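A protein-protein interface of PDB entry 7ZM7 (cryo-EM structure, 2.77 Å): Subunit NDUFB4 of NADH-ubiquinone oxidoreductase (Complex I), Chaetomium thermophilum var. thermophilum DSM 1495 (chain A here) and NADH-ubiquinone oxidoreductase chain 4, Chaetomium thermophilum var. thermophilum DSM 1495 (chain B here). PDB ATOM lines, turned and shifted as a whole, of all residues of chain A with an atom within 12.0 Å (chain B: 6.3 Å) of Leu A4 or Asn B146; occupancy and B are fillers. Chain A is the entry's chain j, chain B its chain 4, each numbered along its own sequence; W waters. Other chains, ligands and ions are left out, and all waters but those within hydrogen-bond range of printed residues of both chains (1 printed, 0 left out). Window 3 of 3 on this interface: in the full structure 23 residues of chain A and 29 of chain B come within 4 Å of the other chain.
ND2 of Asn B146 lies close to NE of Arg B492, 3.4 Å away. The side-chain hydroxyl (OG) of Ser B147 is in hydrogen-bond range of the side-chain carboxylate (OD2) of Asp B393 (3.4 Å).
Among the printed residues, pairs that only touch across the chains: Leu A4 with Asn B146 (2.9 Å), His A6 with Asp B393 (3.6 Å), Leu A4 with Thr B149 (3.6 Å), Leu A4 with Ser B147 (3.8 Å) and Gly A3 with Thr B149 (3.97 Å).
Printed residues of chain B within 4 Å of Gly A3: Thr B149. Leu A4 touches just these residues of chain B: Asn B146, Ser B147 and Thr B149. Of the printed residues of chain B, His A6 touches Asp B393. Leu B141 touches none of the printed residues of chain A. No residue of chain A comes within 4 Å of Trp B145. Printed residues of chain A within 4 Å of Asn B146: Leu A4. Of chain A, only Leu A4 comes within 4 Å of Ser B147. No residue of chain A comes within 4 Å of Ile B148. Asp B393 touches one residue of chain A. The nearest residue of chain B that does not touch Leu A4 is Asp B393 (5.2 Å). The nearest printed residue of chain B that does not touch Gly A3 is Ser B147 (4.9 Å).
Among the printed residues, no Asp or Glu carboxylate lies within 4 Å of a Lys or Arg side-chain nitrogen of the other chain.
Water W1 lies within hydrogen-bond range of O of Asp B393 (2.7 Å) and O of Leu A4 (2.9 Å).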
ATOM      1  N   GLY A   3      -9.416  12.252  34.171  1.00  0.00           N
ATOM      2  CA  GLY A   3      -9.665  11.544  32.928  1.00  0.00           C
ATOM      3  C   GLY A   3      -8.504  10.680  32.499  1.00  0.00           C
ATOM      4  O   GLY A   3      -8.140   9.740  33.190  1.00  0.00           O
ATOM      5  N   LEU A   4      -7.931  10.994  31.347  1.00  0.00           N
ATOM      6  CA  LEU A   4      -6.718  10.318  30.915  1.00  0.00           C
ATOM      7  C   LEU A   4      -5.577  10.626  31.870  1.00  0.00           C
ATOM      8  O   LEU A   4      -5.449  11.745  32.369  1.00  0.00           O
ATOM      9  CB  LEU A   4      -6.323  10.749  29.500  1.00  0.00           C
ATOM     10  CG  LEU A   4      -6.908  10.012  28.297  1.00  0.00           C
ATOM     11  CD1 LEU A   4      -6.535   8.540  28.366  1.00  0.00           C
ATOM     12  CD2 LEU A   4      -8.368  10.171  28.247  1.00  0.00           C
ATOM     13  N   GLN A   5      -4.711   9.635  32.062  1.00  0.00           N
ATOM     14  CA  GLN A   5      -3.499   9.913  32.864  1.00  0.00           C
ATOM     15  C   GLN A   5      -2.512  10.655  31.965  1.00  0.00           C
ATOM     16  O   GLN A   5      -2.275  10.210  30.837  1.00  0.00           O
ATOM     17  CB  GLN A   5      -2.904   8.628  33.439  1.00  0.00           C
ATOM     18  CG  GLN A   5      -2.899   7.456  32.469  1.00  0.00           C
ATOM     19  CD  GLN A   5      -2.204   6.253  33.058  1.00  0.00           C
ATOM     20  OE1 GLN A   5      -1.594   6.326  34.122  1.00  0.00           O
ATOM     21  NE2 GLN A   5      -2.289   5.132  32.362  1.00  0.00           N
ATOM     22  N   HIS A   6      -1.981  11.755  32.468  1.00  0.00           N
ATOM     23  CA  HIS A   6      -1.011  12.578  31.725  1.00  0.00           C
ATOM     24  C   HIS A   6       0.411  12.071  31.994  1.00  0.00           C
ATOM     25  O   HIS A   6       0.557  11.139  32.791  1.00  0.00           O
ATOM     26  CB  HIS A   6      -1.242  14.030  32.133  1.00  0.00           C
ATOM     27  CG  HIS A   6      -1.220  14.280  33.601  1.00  0.00           C
ATOM     28  ND1 HIS A   6      -0.052  14.506  34.293  1.00  0.00           N
ATOM     29  CD2 HIS A   6      -2.218  14.379  34.500  1.00  0.00           C
ATOM     30  CE1 HIS A   6      -0.327  14.711  35.561  1.00  0.00           C
ATOM     31  NE2 HIS A   6      -1.648  14.641  35.714  1.00  0.00           N
ATOM     32  N   TYR A   7       1.392  12.624  31.293  1.00  0.00           N
ATOM     33  CA  TYR A   7       2.802  12.253  31.490  1.00  0.00           C
ATOM     34  C   TYR A   7       3.269  12.868  32.805  1.00  0.00           C
ATOM     35  O   TYR A   7       2.632  13.801  33.293  1.00  0.00           O
ATOM     36  CB  TYR A   7       3.640  12.746  30.316  1.00  0.00           C
ATOM     37  CG  TYR A   7       3.410  12.081  28.985  1.00  0.00           C
ATOM     38  CD1 TYR A   7       3.994  10.865  28.691  1.00  0.00           C
ATOM     39  CD2 TYR A   7       2.659  12.691  27.996  1.00  0.00           C
ATOM     40  CE1 TYR A   7       3.806  10.253  27.465  1.00  0.00           C
ATOM     41  CE2 TYR A   7       2.462  12.093  26.763  1.00  0.00           C
ATOM     42  CZ  TYR A   7       3.038  10.868  26.496  1.00  0.00           C
ATOM     43  OH  TYR A   7       2.857  10.257  25.291  1.00  0.00           O
ATOM     44  N   LYS A   8       4.408  12.415  33.322  1.00  0.00           N
ATOM     45  CA  LYS A   8       4.925  12.921  34.619  1.00  0.00           C
ATOM     46  C   LYS A   8       5.428  14.364  34.493  1.00  0.00           C
ATOM     47  O   LYS A   8       6.199  14.638  33.572  1.00  0.00           O
ATOM     48  CB  LYS A   8       5.993  11.967  35.154  1.00  0.00           C
ATOM     49  CG  LYS A   8       5.571  10.504  35.198  1.00  0.00           C
ATOM     50  CD  LYS A   8       6.663   9.577  35.678  1.00  0.00           C
ATOM     51  CE  LYS A   8       6.296   8.116  35.533  1.00  0.00           C
ATOM     52  NZ  LYS A   8       5.010   7.806  36.201  1.00  0.00           N
ATOM     53  N   ILE A   9       4.982  15.249  35.388  1.00  0.00           N
ATOM     54  CA  ILE A   9       5.392  16.687  35.379  1.00  0.00           C
ATOM     55  C   ILE A   9       6.017  17.008  36.730  1.00  0.00           C
ATOM     56  O   ILE A   9       5.427  16.610  37.741  1.00  0.00           O
ATOM     57  CB  ILE A   9       4.178  17.604  35.131  1.00  0.00           C
ATOM     58  CG1 ILE A   9       3.497  17.287  33.802  1.00  0.00           C
ATOM     59  CG2 ILE A   9       4.595  19.065  35.190  1.00  0.00           C
ATOM     60  CD1 ILE A   9       4.275  17.788  32.615  1.00  0.00           C
ATOM     61  N   LYS B  76     -20.084   6.219  20.468  1.00  0.00           N
ATOM     62  CA  LYS B  76     -19.404   7.344  19.841  1.00  0.00           C
ATOM     63  C   LYS B  76     -19.564   7.320  18.336  1.00  0.00           C
ATOM     64  O   LYS B  76     -19.605   8.374  17.699  1.00  0.00           O
ATOM     65  CB  LYS B  76     -17.924   7.326  20.180  1.00  0.00           C
ATOM     66  CG  LYS B  76     -17.587   7.243  21.613  1.00  0.00           C
ATOM     67  CD  LYS B  76     -16.125   6.905  21.752  1.00  0.00           C
ATOM     68  CE  LYS B  76     -15.663   6.997  23.162  1.00  0.00           C
ATOM     69  NZ  LYS B  76     -15.022   8.305  23.359  1.00  0.00           N
ATOM     70  N   LEU B 141     -16.836  16.520  18.230  1.00  0.00           N
ATOM     71  CA  LEU B 141     -16.922  15.154  18.733  1.00  0.00           C
ATOM     72  C   LEU B 141     -15.585  14.432  18.618  1.00  0.00           C
ATOM     73  O   LEU B 141     -15.137  13.783  19.567  1.00  0.00           O
ATOM     74  CB  LEU B 141     -18.007  14.391  17.982  1.00  0.00           C
ATOM     75  CG  LEU B 141     -19.447  14.558  18.469  1.00  0.00           C
ATOM     76  CD1 LEU B 141     -20.307  13.679  17.651  1.00  0.00           C
ATOM     77  CD2 LEU B 141     -19.608  14.222  19.934  1.00  0.00           C
ATOM     78  N   VAL B 142     -14.928  14.542  17.463  1.00  0.00           N
ATOM     79  CA  VAL B 142     -13.665  13.850  17.248  1.00  0.00           C
ATOM     80  C   VAL B 142     -12.581  14.404  18.157  1.00  0.00           C
ATOM     81  O   VAL B 142     -11.715  13.666  18.626  1.00  0.00           O
ATOM     82  CB  VAL B 142     -13.255  13.941  15.770  1.00  0.00           C
ATOM     83  CG1 VAL B 142     -11.930  13.244  15.545  1.00  0.00           C
ATOM     84  CG2 VAL B 142     -14.313  13.327  14.901  1.00  0.00           C
ATOM     85  N   SER B 143     -12.606  15.711  18.415  1.00  0.00           N
ATOM     86  CA  SER B 143     -11.571  16.313  19.246  1.00  0.00           C
ATOM     87  C   SER B 143     -11.551  15.721  20.638  1.00  0.00           C
ATOM     88  O   SER B 143     -10.494  15.629  21.261  1.00  0.00           O
ATOM     89  CB  SER B 143     -11.773  17.818  19.357  1.00  0.00           C
ATOM     90  OG  SER B 143     -12.955  18.109  20.068  1.00  0.00           O
ATOM     91  N   ASN B 144     -12.697  15.331  21.149  1.00  0.00           N
ATOM     92  CA  ASN B 144     -12.825  15.004  22.551  1.00  0.00           C
ATOM     93  C   ASN B 144     -13.142  13.512  22.667  1.00  0.00           C
ATOM     94  O   ASN B 144     -13.825  13.054  23.583  1.00  0.00           O
ATOM     95  CB  ASN B 144     -13.881  15.951  23.121  1.00  0.00           C
ATOM     96  CG  ASN B 144     -13.971  15.939  24.594  1.00  0.00           C
ATOM     97  OD1 ASN B 144     -13.270  15.206  25.269  1.00  0.00           O
ATOM     98  ND2 ASN B 144     -14.761  16.856  25.121  1.00  0.00           N
ATOM     99  N   TRP B 145     -12.653  12.765  21.661  1.00  0.00           N
ATOM    100  CA  TRP B 145     -12.945  11.312  21.508  1.00  0.00           C
ATOM    101  C   TRP B 145     -12.400  10.443  22.634  1.00  0.00           C
ATOM    102  O   TRP B 145     -13.013   9.433  22.905  1.00  0.00           O
ATOM    103  CB  TRP B 145     -12.380  10.840  20.165  1.00  0.00           C
ATOM    104  CG  TRP B 145     -12.858   9.506  19.681  1.00  0.00           C
ATOM    105  CD1 TRP B 145     -12.283   8.290  19.915  1.00  0.00           C
ATOM    106  CD2 TRP B 145     -13.990   9.252  18.831  1.00  0.00           C
ATOM    107  NE1 TRP B 145     -12.991   7.298  19.293  1.00  0.00           N
ATOM    108  CE2 TRP B 145     -14.043   7.858  18.618  1.00  0.00           C
ATOM    109  CE3 TRP B 145     -14.966  10.062  18.240  1.00  0.00           C
ATOM    110  CZ2 TRP B 145     -15.035   7.262  17.842  1.00  0.00           C
ATOM    111  CZ3 TRP B 145     -15.944   9.471  17.473  1.00  0.00           C
ATOM    112  CH2 TRP B 145     -15.974   8.092  17.275  1.00  0.00           C
ATOM    113  N   ASN B 146     -11.239  10.741  23.197  1.00  0.00           N
ATOM    114  CA  ASN B 146     -10.751   9.792  24.229  1.00  0.00           C
ATOM    115  C   ASN B 146     -10.774  10.496  25.573  1.00  0.00           C
ATOM    116  O   ASN B 146     -10.674   9.782  26.566  1.00  0.00           O
ATOM    117  CB  ASN B 146      -9.347   9.312  23.863  1.00  0.00           C
ATOM    118  CG  ASN B 146      -9.275   8.728  22.470  1.00  0.00           C
ATOM    119  OD1 ASN B 146     -10.023   7.811  22.138  1.00  0.00           O
ATOM    120  ND2 ASN B 146      -8.381   9.248  21.648  1.00  0.00           N
ATOM    121  N   SER B 147     -11.115  11.781  25.612  1.00  0.00           N
ATOM    122  CA  SER B 147     -10.927  12.592  26.798  1.00  0.00           C
ATOM    123  C   SER B 147     -12.111  12.576  27.755  1.00  0.00           C
ATOM    124  O   SER B 147     -11.982  13.102  28.865  1.00  0.00           O
ATOM    125  CB  SER B 147     -10.661  14.031  26.363  1.00  0.00           C
ATOM    126  OG  SER B 147      -9.465  14.131  25.623  1.00  0.00           O
ATOM    127  N   ILE B 148     -13.252  12.011  27.370  1.00  0.00           N
ATOM    128  CA  ILE B 148     -14.444  12.115  28.206  1.00  0.00           C
ATOM    129  C   ILE B 148     -14.471  11.019  29.268  1.00  0.00           C
ATOM    130  O   ILE B 148     -14.697  11.297  30.452  1.00  0.00           O
ATOM    131  CB  ILE B 148     -15.714  12.139  27.338  1.00  0.00           C
ATOM    132  CG1 ILE B 148     -15.725  13.426  26.525  1.00  0.00           C
ATOM    133  CG2 ILE B 148     -16.954  12.039  28.168  1.00  0.00           C
ATOM    134  CD1 ILE B 148     -15.609  14.655  27.378  1.00  0.00           C
ATOM    135  N   THR B 149     -14.273   9.770  28.868  1.00  0.00           N
ATOM    136  CA  THR B 149     -13.955   8.668  29.777  1.00  0.00           C
ATOM    137  C   THR B 149     -15.074   8.244  30.726  1.00  0.00           C
ATOM    138  O   THR B 149     -14.991   7.170  31.323  1.00  0.00           O
ATOM    139  CB  THR B 149     -12.725   8.997  30.652  1.00  0.00           C
ATOM    140  OG1 THR B 149     -13.078   9.968  31.644  1.00  0.00           O
ATOM    141  CG2 THR B 149     -11.543   9.518  29.826  1.00  0.00           C
ATOM    142  N   ASP B 393      -4.078  17.519  27.801  1.00  0.00           N
ATOM    143  CA  ASP B 393      -4.068  16.067  27.760  1.00  0.00           C
ATOM    144  C   ASP B 393      -2.738  15.494  28.211  1.00  0.00           C
ATOM    145  O   ASP B 393      -2.709  14.462  28.883  1.00  0.00           O
ATOM    146  CB  ASP B 393      -4.371  15.570  26.349  1.00  0.00           C
ATOM    147  CG  ASP B 393      -5.839  15.347  26.120  1.00  0.00           C
ATOM    148  OD1 ASP B 393      -6.627  15.607  27.052  1.00  0.00           O
ATOM    149  OD2 ASP B 393      -6.202  14.895  25.015  1.00  0.00           O
ATOM    150  N   THR B 490      -1.328  12.858  17.485  1.00  0.00           N
ATOM    151  CA  THR B 490      -1.851  11.538  17.069  1.00  0.00           C
ATOM    152  C   THR B 490      -2.473  11.736  15.692  1.00  0.00           C
ATOM    153  O   THR B 490      -2.516  12.881  15.238  1.00  0.00           O
ATOM    154  CB  THR B 490      -2.822  10.987  18.119  1.00  0.00           C
ATOM    155  OG1 THR B 490      -3.964  11.840  18.179  1.00  0.00           O
ATOM    156  CG2 THR B 490      -2.196  10.850  19.489  1.00  0.00           C
ATOM    157  N   ARG B 492      -5.522  11.407  15.132  1.00  0.00           N
ATOM    158  CA  ARG B 492      -6.787  12.124  15.402  1.00  0.00           C
ATOM    159  C   ARG B 492      -6.475  13.614  15.544  1.00  0.00           C
ATOM    160  O   ARG B 492      -7.180  14.415  14.913  1.00  0.00           O
ATOM    161  CB  ARG B 492      -7.397  11.581  16.695  1.00  0.00           C
ATOM    162  CG  ARG B 492      -8.850  11.964  16.922  1.00  0.00           C
ATOM    163  CD  ARG B 492      -9.323  11.429  18.257  1.00  0.00           C
ATOM    164  NE  ARG B 492      -8.406  11.745  19.341  1.00  0.00           N
ATOM    165  CZ  ARG B 492      -8.331  12.925  19.945  1.00  0.00           C
ATOM    166  NH1 ARG B 492      -7.463  13.119  20.921  1.00  0.00           N
ATOM    167  NH2 ARG B 492      -9.110  13.917  19.558  1.00  0.00           N
HETATM  168  O   HOH W   1      -4.732  13.749  30.464  1.00  0.00           O
